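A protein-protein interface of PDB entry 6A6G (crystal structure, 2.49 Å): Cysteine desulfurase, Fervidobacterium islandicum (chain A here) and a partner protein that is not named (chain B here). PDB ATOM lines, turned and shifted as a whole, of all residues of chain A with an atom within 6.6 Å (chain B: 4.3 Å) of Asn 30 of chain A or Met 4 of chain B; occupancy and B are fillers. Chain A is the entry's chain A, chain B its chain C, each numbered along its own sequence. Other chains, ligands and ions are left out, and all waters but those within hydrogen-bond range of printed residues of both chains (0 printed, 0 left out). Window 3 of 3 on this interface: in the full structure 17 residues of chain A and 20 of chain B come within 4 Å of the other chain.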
ATOM      1  N   ASN A  28     -15.082  26.621  26.155  1.00  0.00           N
ATOM      2  CA  ASN A  28     -13.885  26.389  25.405  1.00  0.00           C
ATOM      3  C   ASN A  28     -13.625  24.908  25.296  1.00  0.00           C
ATOM      4  O   ASN A  28     -13.942  24.145  26.200  1.00  0.00           O
ATOM      5  CB  ASN A  28     -12.723  27.082  26.098  1.00  0.00           C
ATOM      6  CG  ASN A  28     -12.752  28.582  25.895  1.00  0.00           C
ATOM      7  OD1 ASN A  28     -12.884  29.072  24.769  1.00  0.00           O
ATOM      8  ND2 ASN A  28     -12.626  29.325  26.985  1.00  0.00           N
ATOM      9  N   ILE A  29     -13.074  24.493  24.159  1.00  0.00           N
ATOM     10  CA  ILE A  29     -12.719  23.070  23.926  1.00  0.00           C
ATOM     11  C   ILE A  29     -11.261  23.074  23.516  1.00  0.00           C
ATOM     12  O   ILE A  29     -10.905  23.611  22.457  1.00  0.00           O
ATOM     13  CB  ILE A  29     -13.581  22.399  22.824  1.00  0.00           C
ATOM     14  CG1 ILE A  29     -15.084  22.481  23.170  1.00  0.00           C
ATOM     15  CG2 ILE A  29     -13.157  20.953  22.621  1.00  0.00           C
ATOM     16  CD1 ILE A  29     -16.004  22.386  21.960  1.00  0.00           C
ATOM     17  N   ASN A  30     -10.425  22.516  24.389  1.00  0.00           N
ATOM     18  CA  ASN A  30      -8.987  22.490  24.184  1.00  0.00           C
ATOM     19  C   ASN A  30      -8.485  23.844  23.772  1.00  0.00           C
ATOM     20  O   ASN A  30      -7.813  23.993  22.763  1.00  0.00           O
ATOM     21  CB  ASN A  30      -8.629  21.438  23.135  1.00  0.00           C
ATOM     22  CG  ASN A  30      -8.984  20.037  23.591  1.00  0.00           C
ATOM     23  OD1 ASN A  30      -8.802  19.676  24.773  1.00  0.00           O
ATOM     24  ND2 ASN A  30      -9.530  19.245  22.671  1.00  0.00           N
ATOM     25  N   GLY A  31      -8.844  24.843  24.560  1.00  0.00           N
ATOM     26  CA  GLY A  31      -8.405  26.201  24.322  1.00  0.00           C
ATOM     27  C   GLY A  31      -9.202  27.014  23.336  1.00  0.00           C
ATOM     28  O   GLY A  31      -9.023  28.218  23.298  1.00  0.00           O
ATOM     29  N   LYS A  32     -10.076  26.399  22.531  1.00  0.00           N
ATOM     30  CA  LYS A  32     -10.849  27.165  21.524  1.00  0.00           C
ATOM     31  C   LYS A  32     -12.342  27.340  21.847  1.00  0.00           C
ATOM     32  O   LYS A  32     -12.981  26.464  22.421  1.00  0.00           O
ATOM     33  CB  LYS A  32     -10.672  26.536  20.153  1.00  0.00           C
ATOM     34  CG  LYS A  32      -9.234  26.592  19.689  1.00  0.00           C
ATOM     35  CD  LYS A  32      -9.088  26.051  18.305  1.00  0.00           C
ATOM     36  CE  LYS A  32      -7.634  25.810  17.992  1.00  0.00           C
ATOM     37  NZ  LYS A  32      -7.537  25.373  16.575  1.00  0.00           N
ATOM     38  N   HIS A 360     -14.969  14.707  14.415  1.00  0.00           N
ATOM     39  CA  HIS A 360     -14.181  14.556  15.641  1.00  0.00           C
ATOM     40  C   HIS A 360     -13.090  15.591  15.705  1.00  0.00           C
ATOM     41  O   HIS A 360     -12.961  16.314  16.704  1.00  0.00           O
ATOM     42  CB  HIS A 360     -13.569  13.172  15.729  1.00  0.00           C
ATOM     43  CG  HIS A 360     -12.941  12.902  17.047  1.00  0.00           C
ATOM     44  ND1 HIS A 360     -13.445  11.977  17.928  1.00  0.00           N
ATOM     45  CD2 HIS A 360     -11.874  13.472  17.662  1.00  0.00           C
ATOM     46  CE1 HIS A 360     -12.719  11.986  19.033  1.00  0.00           C
ATOM     47  NE2 HIS A 360     -11.770  12.897  18.906  1.00  0.00           N
ATOM     48  N   ASP A 363     -14.314  19.013  16.091  1.00  0.00           N
ATOM     49  CA  ASP A 363     -14.664  19.295  17.470  1.00  0.00           C
ATOM     50  C   ASP A 363     -13.452  19.404  18.388  1.00  0.00           C
ATOM     51  O   ASP A 363     -13.319  20.372  19.129  1.00  0.00           O
ATOM     52  CB  ASP A 363     -15.590  18.243  18.047  1.00  0.00           C
ATOM     53  CG  ASP A 363     -15.871  18.484  19.529  1.00  0.00           C
ATOM     54  OD1 ASP A 363     -16.640  19.430  19.816  1.00  0.00           O
ATOM     55  OD2 ASP A 363     -15.317  17.747  20.391  1.00  0.00           O
ATOM     56  N   GLU A 364     -12.592  18.405  18.350  1.00  0.00           N
ATOM     57  CA  GLU A 364     -11.555  18.287  19.356  1.00  0.00           C
ATOM     58  C   GLU A 364     -10.480  19.339  19.158  1.00  0.00           C
ATOM     59  O   GLU A 364      -9.871  19.797  20.133  1.00  0.00           O
ATOM     60  CB  GLU A 364     -10.945  16.862  19.357  1.00  0.00           C
ATOM     61  CG  GLU A 364     -10.041  16.624  20.546  1.00  0.00           C
ATOM     62  CD  GLU A 364      -9.621  15.177  20.738  1.00  0.00           C
ATOM     63  OE1 GLU A 364      -9.574  14.748  21.925  1.00  0.00           O
ATOM     64  OE2 GLU A 364      -9.321  14.477  19.722  1.00  0.00           O
ATOM     65  N   ASN A 365     -10.245  19.716  17.897  1.00  0.00           N
ATOM     66  CA  ASN A 365      -9.140  20.598  17.550  1.00  0.00           C
ATOM     67  C   ASN A 365      -9.581  21.972  17.137  1.00  0.00           C
ATOM     68  O   ASN A 365      -8.760  22.894  17.097  1.00  0.00           O
ATOM     69  CB  ASN A 365      -8.382  20.050  16.368  1.00  0.00           C
ATOM     70  CG  ASN A 365      -7.645  18.783  16.674  1.00  0.00           C
ATOM     71  OD1 ASN A 365      -8.214  17.829  17.183  1.00  0.00           O
ATOM     72  ND2 ASN A 365      -6.361  18.752  16.310  1.00  0.00           N
ATOM     73  N   TRP A 423      -4.273  16.267   7.314  1.00  0.00           N
ATOM     74  CA  TRP A 423      -4.038  15.224   8.322  1.00  0.00           C
ATOM     75  C   TRP A 423      -4.078  13.778   7.747  1.00  0.00           C
ATOM     76  O   TRP A 423      -3.236  12.940   8.097  1.00  0.00           O
ATOM     77  CB  TRP A 423      -5.035  15.367   9.489  1.00  0.00           C
ATOM     78  CG  TRP A 423      -4.804  14.339  10.578  1.00  0.00           C
ATOM     79  CD1 TRP A 423      -5.562  13.228  10.835  1.00  0.00           C
ATOM     80  CD2 TRP A 423      -3.707  14.301  11.505  1.00  0.00           C
ATOM     81  NE1 TRP A 423      -5.005  12.501  11.862  1.00  0.00           N
ATOM     82  CE2 TRP A 423      -3.867  13.136  12.293  1.00  0.00           C
ATOM     83  CE3 TRP A 423      -2.607  15.136  11.743  1.00  0.00           C
ATOM     84  CZ2 TRP A 423      -2.976  12.790  13.309  1.00  0.00           C
ATOM     85  CZ3 TRP A 423      -1.712  14.788  12.746  1.00  0.00           C
ATOM     86  CH2 TRP A 423      -1.906  13.621  13.518  1.00  0.00           C
ATOM     87  N   HIS B   3      -1.358  15.100  18.118  1.00  0.00           N
ATOM     88  CA  HIS B   3      -2.689  14.507  17.950  1.00  0.00           C
ATOM     89  C   HIS B   3      -3.270  14.292  19.331  1.00  0.00           C
ATOM     90  O   HIS B   3      -2.569  14.357  20.367  1.00  0.00           O
ATOM     91  CB  HIS B   3      -2.622  13.113  17.287  1.00  0.00           C
ATOM     92  CG  HIS B   3      -1.798  12.146  18.078  1.00  0.00           C
ATOM     93  ND1 HIS B   3      -0.460  11.942  17.818  1.00  0.00           N
ATOM     94  CD2 HIS B   3      -2.082  11.436  19.195  1.00  0.00           C
ATOM     95  CE1 HIS B   3       0.022  11.090  18.701  1.00  0.00           C
ATOM     96  NE2 HIS B   3      -0.934  10.781  19.559  1.00  0.00           N
ATOM     97  N   MET B   4      -4.551  13.978  19.332  1.00  0.00           N
ATOM     98  CA  MET B   4      -5.193  13.535  20.519  1.00  0.00           C
ATOM     99  C   MET B   4      -5.592  12.059  20.352  1.00  0.00           C
ATOM    100  O   MET B   4      -4.751  11.199  20.520  1.00  0.00           O
ATOM    101  CB  MET B   4      -6.269  14.549  20.888  1.00  0.00           C
ATOM    102  CG  MET B   4      -5.604  15.692  21.632  1.00  0.00           C
ATOM    103  SD  MET B   4      -6.521  17.217  21.695  1.00  0.00           S
ATOM    104  CE  MET B   4      -6.187  17.852  20.047  1.00  0.00           C
ATOM    105  N   ILE B   5      -6.812  11.742  19.967  1.00  0.00           N
ATOM    106  CA  ILE B   5      -7.205  10.341  19.786  1.00  0.00           C
ATOM    107  C   ILE B   5      -6.454   9.606  18.662  1.00  0.00           C
ATOM    108  O   ILE B   5      -6.209   8.421  18.779  1.00  0.00           O
ATOM    109  CB  ILE B   5      -8.719  10.258  19.518  1.00  0.00           C
ATOM    110  CG1 ILE B   5      -9.198   8.830  19.675  1.00  0.00           C
ATOM    111  CG2 ILE B   5      -9.075  10.837  18.136  1.00  0.00           C
ATOM    112  CD1 ILE B   5     -10.705   8.744  19.666  1.00  0.00           C
ATOM    113  N   TYR B   6      -6.147  10.295  17.561  1.00  0.00           N
ATOM    114  CA  TYR B   6      -5.561   9.652  16.385  1.00  0.00           C
ATOM    115  C   TYR B   6      -4.027   9.394  16.571  1.00  0.00           C
ATOM    116  O   TYR B   6      -3.179  10.084  16.005  1.00  0.00           O
ATOM    117  CB  TYR B   6      -5.855  10.479  15.110  1.00  0.00           C
ATOM    118  CG  TYR B   6      -7.310  10.491  14.799  1.00  0.00           C
ATOM    119  CD1 TYR B   6      -7.937   9.359  14.274  1.00  0.00           C
ATOM    120  CD2 TYR B   6      -8.081  11.584  15.106  1.00  0.00           C
ATOM    121  CE1 TYR B   6      -9.293   9.334  14.034  1.00  0.00           C
ATOM    122  CE2 TYR B   6      -9.435  11.573  14.879  1.00  0.00           C
ATOM    123  CZ  TYR B   6     -10.045  10.464  14.337  1.00  0.00           C
ATOM    124  OH  TYR B   6     -11.390  10.506  14.094  1.00  0.00           O
ATOM    125  N   TYR B 117     -13.493   8.489  24.954  1.00  0.00           N
ATOM    126  CA  TYR B 117     -14.434   9.157  24.041  1.00  0.00           C
ATOM    127  C   TYR B 117     -15.735   8.364  23.909  1.00  0.00           C
ATOM    128  O   TYR B 117     -15.849   7.491  23.053  1.00  0.00           O
ATOM    129  CB  TYR B 117     -13.796   9.384  22.686  1.00  0.00           C
ATOM    130  CG  TYR B 117     -12.535  10.204  22.769  1.00  0.00           C
ATOM    131  CD1 TYR B 117     -11.307   9.605  23.086  1.00  0.00           C
ATOM    132  CD2 TYR B 117     -12.559  11.564  22.534  1.00  0.00           C
ATOM    133  CE1 TYR B 117     -10.136  10.334  23.150  1.00  0.00           C
ATOM    134  CE2 TYR B 117     -11.389  12.313  22.606  1.00  0.00           C
ATOM    135  CZ  TYR B 117     -10.173  11.685  22.912  1.00  0.00           C
ATOM    136  OH  TYR B 117      -9.023  12.418  22.948  1.00  0.00           O
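ND2 of Asn 30 of chain A sits at hydrogen-bond distance from O of Glu 364 of chain A, 2.6 Å away. The backbone carbonyl oxygen (O) of Asn 365 of chain A is in hydrogen-bond range of the side-chain amino group (NZ) of Lys 32 of chain A, 2.8 Å away. A ring nitrogen (NE2) of His 360 of chain A is in hydrogen-bond range of the side-chain carboxylate (OE2) of Glu 364 of chain A, 3.0 Å away.
Of the 10 printed residues of chain A, 5 touch a printed residue of chain B. Hydrophobic or aromatic side chains of chain A that line the printed part of chain B: His 360 and Trp 423. Of the 5 printed residues of chain B, 5 touch a printed residue of chain A. Printed residues of chain B that touch a printed residue of chain A: His 3, Met 4, Ile 5, Tyr 6 and Tyr 117. Hydrophobic or aromatic side chains of chain B that line the printed part of chain A: His 3, Met 4, Ile 5, Tyr 6 and Tyr 117. Among the printed residues, 10 pairs touch across the chains. Among the printed residues, no Asp or Glu carboxylate lies within 4 Å of a Lys or Arg side-chain nitrogen of the other chain.
Of chain B, only Met 4 (3.8 Å) comes within 4 Å of Asn 30 of chain A. Met 4 of chain B touches just these residues of chain A: Asn 30, Glu 364 and Asn 365. Of the printed residues of chain A, Tyr 117 of chain B touches His 360 (3.5 Å) and Glu 364 (2.6 Å). Of the printed residues of chain B, His 360 of chain A touches Ile 5 (3.5 Å), Tyr 6 (3.8 Å) and Tyr 117 (3.5 Å). Of the printed residues of chain B, Asn 365 of chain A touches Met 4. Of the printed residues of chain B, Trp 423 of chain A touches His 3 (3.9 Å) and Tyr 6 (3.8 Å). Gly 31 of chain A touches none of the printed residues of chain B.
The side-chain amide nitrogen (ND2) of Asn 30 of chain A lies within hydrogen-bond range of the side-chain sulfur (SD) of Met 4 of chain B (3.8 Å). The side-chain carboxylate of Glu 364 of chain A sits at hydrogen-bond distance from the side-chain hydroxyl of Tyr 117 of chain B.
Among the printed residues, merely in contact across the chains: His 360 of chain A with Ile 5 of chain B (3.5 Å), His 360 of chain A with Tyr 6 of chain B (3.8 Å), His 360 of chain A with Tyr 117 of chain B (3.5 Å), Glu 364 of chain A with Met 4 of chain B (3.3 Å), Glu 364 of chain A with Ile 5 of chain B (3.7 Å), Asn 365 of chain A with Met 4 of chain B (3.5 Å), Trp 423 of chain A with His 3 of chain B (3.9 Å) and Trp 423 of chain A with Tyr 6 of chain B (3.8 Å).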
